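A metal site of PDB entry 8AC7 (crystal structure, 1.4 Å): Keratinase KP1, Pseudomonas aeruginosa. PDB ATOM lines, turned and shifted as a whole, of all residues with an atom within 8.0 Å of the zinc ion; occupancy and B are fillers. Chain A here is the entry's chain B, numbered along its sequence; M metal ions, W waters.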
ATOM      1  N   ILE A 354     -15.755  18.253   5.632  1.00  0.00           N
ATOM      2  CA  ILE A 354     -15.594  18.899   4.336  1.00  0.00           C
ATOM      3  C   ILE A 354     -16.606  18.271   3.389  1.00  0.00           C
ATOM      4  O   ILE A 354     -16.706  17.043   3.312  1.00  0.00           O
ATOM      5  CB  ILE A 354     -14.157  18.717   3.804  1.00  0.00           C
ATOM      6  CG1 ILE A 354     -13.151  19.381   4.743  1.00  0.00           C
ATOM      7  CG2 ILE A 354     -14.042  19.251   2.372  1.00  0.00           C
ATOM      8  CD1 ILE A 354     -11.692  19.040   4.427  1.00  0.00           C
ATOM      9  N   TYR A 355     -17.347  19.099   2.649  1.00  0.00           N
ATOM     10  CA  TYR A 355     -18.340  18.564   1.731  1.00  0.00           C
ATOM     11  C   TYR A 355     -17.697  17.539   0.800  1.00  0.00           C
ATOM     12  O   TYR A 355     -16.646  17.784   0.211  1.00  0.00           O
ATOM     13  CB  TYR A 355     -18.948  19.687   0.886  1.00  0.00           C
ATOM     14  CG  TYR A 355     -19.887  20.647   1.600  1.00  0.00           C
ATOM     15  CD1 TYR A 355     -20.560  21.623   0.879  1.00  0.00           C
ATOM     16  CD2 TYR A 355     -20.098  20.589   2.978  1.00  0.00           C
ATOM     17  CE1 TYR A 355     -21.397  22.501   1.483  1.00  0.00           C
ATOM     18  CE2 TYR A 355     -20.958  21.480   3.598  1.00  0.00           C
ATOM     19  CZ  TYR A 355     -21.595  22.435   2.837  1.00  0.00           C
ATOM     20  OH  TYR A 355     -22.456  23.346   3.417  1.00  0.00           O
ATOM     21  N   ASP A 356     -18.363  16.389   0.647  1.00  0.00           N
ATOM     22  CA  ASP A 356     -17.822  15.260  -0.119  1.00  0.00           C
ATOM     23  C   ASP A 356     -18.141  15.398  -1.612  1.00  0.00           C
ATOM     24  O   ASP A 356     -18.843  14.593  -2.218  1.00  0.00           O
ATOM     25  CB  ASP A 356     -18.395  13.961   0.464  1.00  0.00           C
ATOM     26  CG  ASP A 356     -17.876  12.727  -0.228  1.00  0.00           C
ATOM     27  OD1 ASP A 356     -16.700  12.683  -0.620  1.00  0.00           O
ATOM     28  OD2 ASP A 356     -18.651  11.754  -0.348  1.00  0.00           O
ATOM     29  N   GLY A 357     -17.572  16.452  -2.222  1.00  0.00           N
ATOM     30  CA  GLY A 357     -17.869  16.765  -3.612  1.00  0.00           C
ATOM     31  C   GLY A 357     -17.471  15.698  -4.609  1.00  0.00           C
ATOM     32  O   GLY A 357     -18.025  15.625  -5.711  1.00  0.00           O
ATOM     33  N   ASP A 358     -16.479  14.869  -4.270  1.00  0.00           N
ATOM     34  CA  ASP A 358     -16.044  13.793  -5.153  1.00  0.00           C
ATOM     35  C   ASP A 358     -16.803  12.487  -4.916  1.00  0.00           C
ATOM     36  O   ASP A 358     -16.500  11.493  -5.579  1.00  0.00           O
ATOM     37  CB  ASP A 358     -14.532  13.550  -5.056  1.00  0.00           C
ATOM     38  CG  ASP A 358     -14.063  13.108  -3.681  1.00  0.00           C
ATOM     39  OD1 ASP A 358     -14.909  12.881  -2.781  1.00  0.00           O
ATOM     40  OD2 ASP A 358     -12.837  12.978  -3.491  1.00  0.00           O
ATOM     41  N   GLY A 359     -17.768  12.474  -4.001  1.00  0.00           N
ATOM     42  CA  GLY A 359     -18.522  11.256  -3.743  1.00  0.00           C
ATOM     43  C   GLY A 359     -17.737  10.118  -3.117  1.00  0.00           C
ATOM     44  O   GLY A 359     -18.238   8.993  -3.082  1.00  0.00           O
ATOM     45  N   SER A 360     -16.519  10.386  -2.623  1.00  0.00           N
ATOM     46  CA  SER A 360     -15.664   9.327  -2.104  1.00  0.00           C
ATOM     47  C   SER A 360     -16.281   8.603  -0.905  1.00  0.00           C
ATOM     48  O   SER A 360     -16.006   7.419  -0.691  1.00  0.00           O
ATOM     49  CB  SER A 360     -14.296   9.903  -1.719  1.00  0.00           C
ATOM     50  OG  SER A 360     -14.408  10.871  -0.672  1.00  0.00           O
ATOM     51  N   ASP A 361     -17.103   9.301  -0.115  1.00  0.00           N
ATOM     52  CA  ASP A 361     -17.703   8.724   1.084  1.00  0.00           C
ATOM     53  C   ASP A 361     -19.131   8.260   0.872  1.00  0.00           C
ATOM     54  O   ASP A 361     -19.494   7.158   1.306  1.00  0.00           O
ATOM     55  CB  ASP A 361     -17.695   9.743   2.227  1.00  0.00           C
ATOM     56  CG  ASP A 361     -16.291  10.138   2.659  1.00  0.00           C
ATOM     57  OD1 ASP A 361     -15.451   9.250   2.878  1.00  0.00           O
ATOM     58  OD2 ASP A 361     -16.038  11.361   2.760  1.00  0.00           O
ATOM     59  N   PHE A 362     -19.953   9.067   0.213  1.00  0.00           N
ATOM     60  CA  PHE A 362     -21.379   8.826   0.152  1.00  0.00           C
ATOM     61  C   PHE A 362     -21.928   8.603  -1.256  1.00  0.00           C
ATOM     62  O   PHE A 362     -23.146   8.431  -1.406  1.00  0.00           O
ATOM     63  CB  PHE A 362     -22.142   9.947   0.879  1.00  0.00           C
ATOM     64  CG  PHE A 362     -21.564  10.284   2.222  1.00  0.00           C
ATOM     65  CD1 PHE A 362     -20.819  11.443   2.396  1.00  0.00           C
ATOM     66  CD2 PHE A 362     -21.733   9.434   3.307  1.00  0.00           C
ATOM     67  CE1 PHE A 362     -20.271  11.752   3.632  1.00  0.00           C
ATOM     68  CE2 PHE A 362     -21.190   9.735   4.543  1.00  0.00           C
ATOM     69  CZ  PHE A 362     -20.454  10.908   4.700  1.00  0.00           C
ATOM     70  N   GLY A 363     -21.088   8.588  -2.285  1.00  0.00           N
ATOM     71  CA  GLY A 363     -21.504   8.228  -3.627  1.00  0.00           C
ATOM     72  C   GLY A 363     -22.239   9.296  -4.412  1.00  0.00           C
ATOM     73  O   GLY A 363     -22.634   9.032  -5.549  1.00  0.00           O
ATOM     74  N   LEU A 364     -22.438  10.485  -3.861  1.00  0.00           N
ATOM     75  CA  LEU A 364     -23.068  11.586  -4.568  1.00  0.00           C
ATOM     76  C   LEU A 364     -21.990  12.593  -4.943  1.00  0.00           C
ATOM     77  O   LEU A 364     -21.306  13.129  -4.063  1.00  0.00           O
ATOM     78  CB  LEU A 364     -24.137  12.254  -3.698  1.00  0.00           C
ATOM     79  CG  LEU A 364     -24.902  13.428  -4.318  1.00  0.00           C
ATOM     80  CD1 LEU A 364     -25.592  13.026  -5.615  1.00  0.00           C
ATOM     81  CD2 LEU A 364     -25.905  14.008  -3.333  1.00  0.00           C
ATOM     82  N   SER A 370     -16.171  20.308  -8.331  1.00  0.00           N
ATOM     83  CA  SER A 370     -16.440  20.114  -6.912  1.00  0.00           C
ATOM     84  C   SER A 370     -15.356  19.257  -6.257  1.00  0.00           C
ATOM     85  O   SER A 370     -15.004  19.488  -5.089  1.00  0.00           O
ATOM     86  CB  SER A 370     -17.810  19.454  -6.743  1.00  0.00           C
ATOM     87  OG  SER A 370     -18.841  20.274  -7.257  1.00  0.00           O
ATOM     88  N   ALA A 371     -14.818  18.279  -6.976  1.00  0.00           N
ATOM     89  CA  ALA A 371     -13.743  17.475  -6.410  1.00  0.00           C
ATOM     90  C   ALA A 371     -12.508  18.317  -6.128  1.00  0.00           C
ATOM     91  O   ALA A 371     -11.884  18.185  -5.070  1.00  0.00           O
ATOM     92  CB  ALA A 371     -13.414  16.301  -7.332  1.00  0.00           C
ATOM     93  N   GLU A 374     -13.078  20.382  -2.915  1.00  0.00           N
ATOM     94  CA  GLU A 374     -12.907  19.508  -1.759  1.00  0.00           C
ATOM     95  C   GLU A 374     -11.435  19.233  -1.490  1.00  0.00           C
ATOM     96  O   GLU A 374     -10.991  19.263  -0.330  1.00  0.00           O
ATOM     97  CB  GLU A 374     -13.667  18.204  -2.017  1.00  0.00           C
ATOM     98  CG  GLU A 374     -13.574  17.162  -0.920  1.00  0.00           C
ATOM     99  CD  GLU A 374     -14.219  15.846  -1.330  1.00  0.00           C
ATOM    100  OE1 GLU A 374     -14.443  15.661  -2.538  1.00  0.00           O
ATOM    101  OE2 GLU A 374     -14.497  14.998  -0.445  1.00  0.00           O
ATOM    102  N   ARG A 375     -10.673  18.964  -2.549  1.00  0.00           N
ATOM    103  CA  ARG A 375      -9.258  18.639  -2.401  1.00  0.00           C
ATOM    104  C   ARG A 375      -8.483  19.829  -1.821  1.00  0.00           C
ATOM    105  O   ARG A 375      -7.565  19.634  -1.011  1.00  0.00           O
ATOM    106  CB  ARG A 375      -8.696  18.218  -3.757  1.00  0.00           C
ATOM    107  CG  ARG A 375      -7.319  17.569  -3.702  1.00  0.00           C
ATOM    108  CD  ARG A 375      -6.984  16.925  -5.051  1.00  0.00           C
ATOM    109  NE  ARG A 375      -7.980  15.925  -5.437  1.00  0.00           N
ATOM    110  CZ  ARG A 375      -8.826  16.055  -6.462  1.00  0.00           C
ATOM    111  NH1 ARG A 375      -8.801  17.149  -7.206  1.00  0.00           N
ATOM    112  NH2 ARG A 375      -9.689  15.079  -6.736  1.00  0.00           N
ATOM    113  N   GLU A 378      -9.271  19.767   1.851  1.00  0.00           N
ATOM    114  CA  GLU A 378      -8.578  18.638   2.459  1.00  0.00           C
ATOM    115  C   GLU A 378      -7.091  18.926   2.620  1.00  0.00           C
ATOM    116  O   GLU A 378      -6.505  18.655   3.673  1.00  0.00           O
ATOM    117  CB  GLU A 378      -8.769  17.377   1.610  1.00  0.00           C
ATOM    118  CG  GLU A 378     -10.191  16.828   1.631  1.00  0.00           C
ATOM    119  CD  GLU A 378     -10.418  15.725   0.600  1.00  0.00           C
ATOM    120  OE1 GLU A 378     -11.405  14.977   0.735  1.00  0.00           O
ATOM    121  OE2 GLU A 378      -9.614  15.600  -0.352  1.00  0.00           O
ATOM    122  N   GLU A 389     -12.840  14.810   7.466  1.00  0.00           N
ATOM    123  CA  GLU A 389     -13.571  13.715   6.826  1.00  0.00           C
ATOM    124  C   GLU A 389     -14.750  14.298   6.072  1.00  0.00           C
ATOM    125  O   GLU A 389     -15.107  15.464   6.238  1.00  0.00           O
ATOM    126  CB  GLU A 389     -14.032  12.666   7.842  1.00  0.00           C
ATOM    127  CG  GLU A 389     -15.105  13.166   8.801  1.00  0.00           C
ATOM    128  CD  GLU A 389     -15.281  12.215   9.966  1.00  0.00           C
ATOM    129  OE1 GLU A 389     -14.432  12.240  10.882  1.00  0.00           O
ATOM    130  OE2 GLU A 389     -16.254  11.436   9.952  1.00  0.00           O
ATOM    131  N   GLY A 390     -15.355  13.470   5.225  1.00  0.00           N
ATOM    132  CA  GLY A 390     -16.432  13.930   4.391  1.00  0.00           C
ATOM    133  C   GLY A 390     -17.756  14.074   5.121  1.00  0.00           C
ATOM    134  O   GLY A 390     -18.012  13.463   6.163  1.00  0.00           O
ATOM    135  N   THR A 391     -18.609  14.928   4.564  1.00  0.00           N
ATOM    136  CA  THR A 391     -20.000  15.024   4.999  1.00  0.00           C
ATOM    137  C   THR A 391     -20.884  15.077   3.755  1.00  0.00           C
ATOM    138  O   THR A 391     -20.439  15.448   2.669  1.00  0.00           O
ATOM    139  CB  THR A 391     -20.220  16.233   5.916  1.00  0.00           C
ATOM    140  OG1 THR A 391     -21.511  16.130   6.548  1.00  0.00           O
ATOM    141  CG2 THR A 391     -20.155  17.538   5.139  1.00  0.00           C
HETATM  142 ZN    ZN M   1     -14.666  12.984  -0.726  1.00  0.00          ZN
HETATM  143  O   HOH W   1     -14.469  12.797   1.321  1.00  0.00           O
HETATM  144  O   HOH W   2     -12.431  13.025  -0.921  1.00  0.00           O
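Water W2 lies within hydrogen-bond range of OD2 of Asp 358 and OE1 of Glu 378.
Within 4 Å of the zinc ion: Asp 356, Asp 358, Ser 360 and Glu 374.
The backbone NH of Asp 356 sits at hydrogen-bond distance from the backbone carbonyl oxygen of Thr 391 (3.0 Å). The side-chain carboxylate (OD2) of Asp 356 lies within hydrogen-bond range of the backbone NH (N) of Phe 362, at 3.0 Å. The backbone NH (N) of Gly 357 lies within hydrogen-bond range of the side-chain carboxylate (OE1) of Glu 374, at 3.2 Å. The side-chain carboxylate (OD2) of Asp 356 sits at hydrogen-bond distance from the backbone NH (N) of Asp 361 (2.9 Å).
OE2 of Glu 374 binds the zinc ion (2.0 Å). The side-chain carboxylate (OD1) of Asp 356 binds the zinc ion. Water W1 binds the zinc ion (2.1 Å). OD1 of Asp 358 is bound to the zinc ion (2.1 Å). OG of Ser 360 is bound to the zinc ion, at 2.1 Å. The zinc ion is bound by water W2 (2.2 Å).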
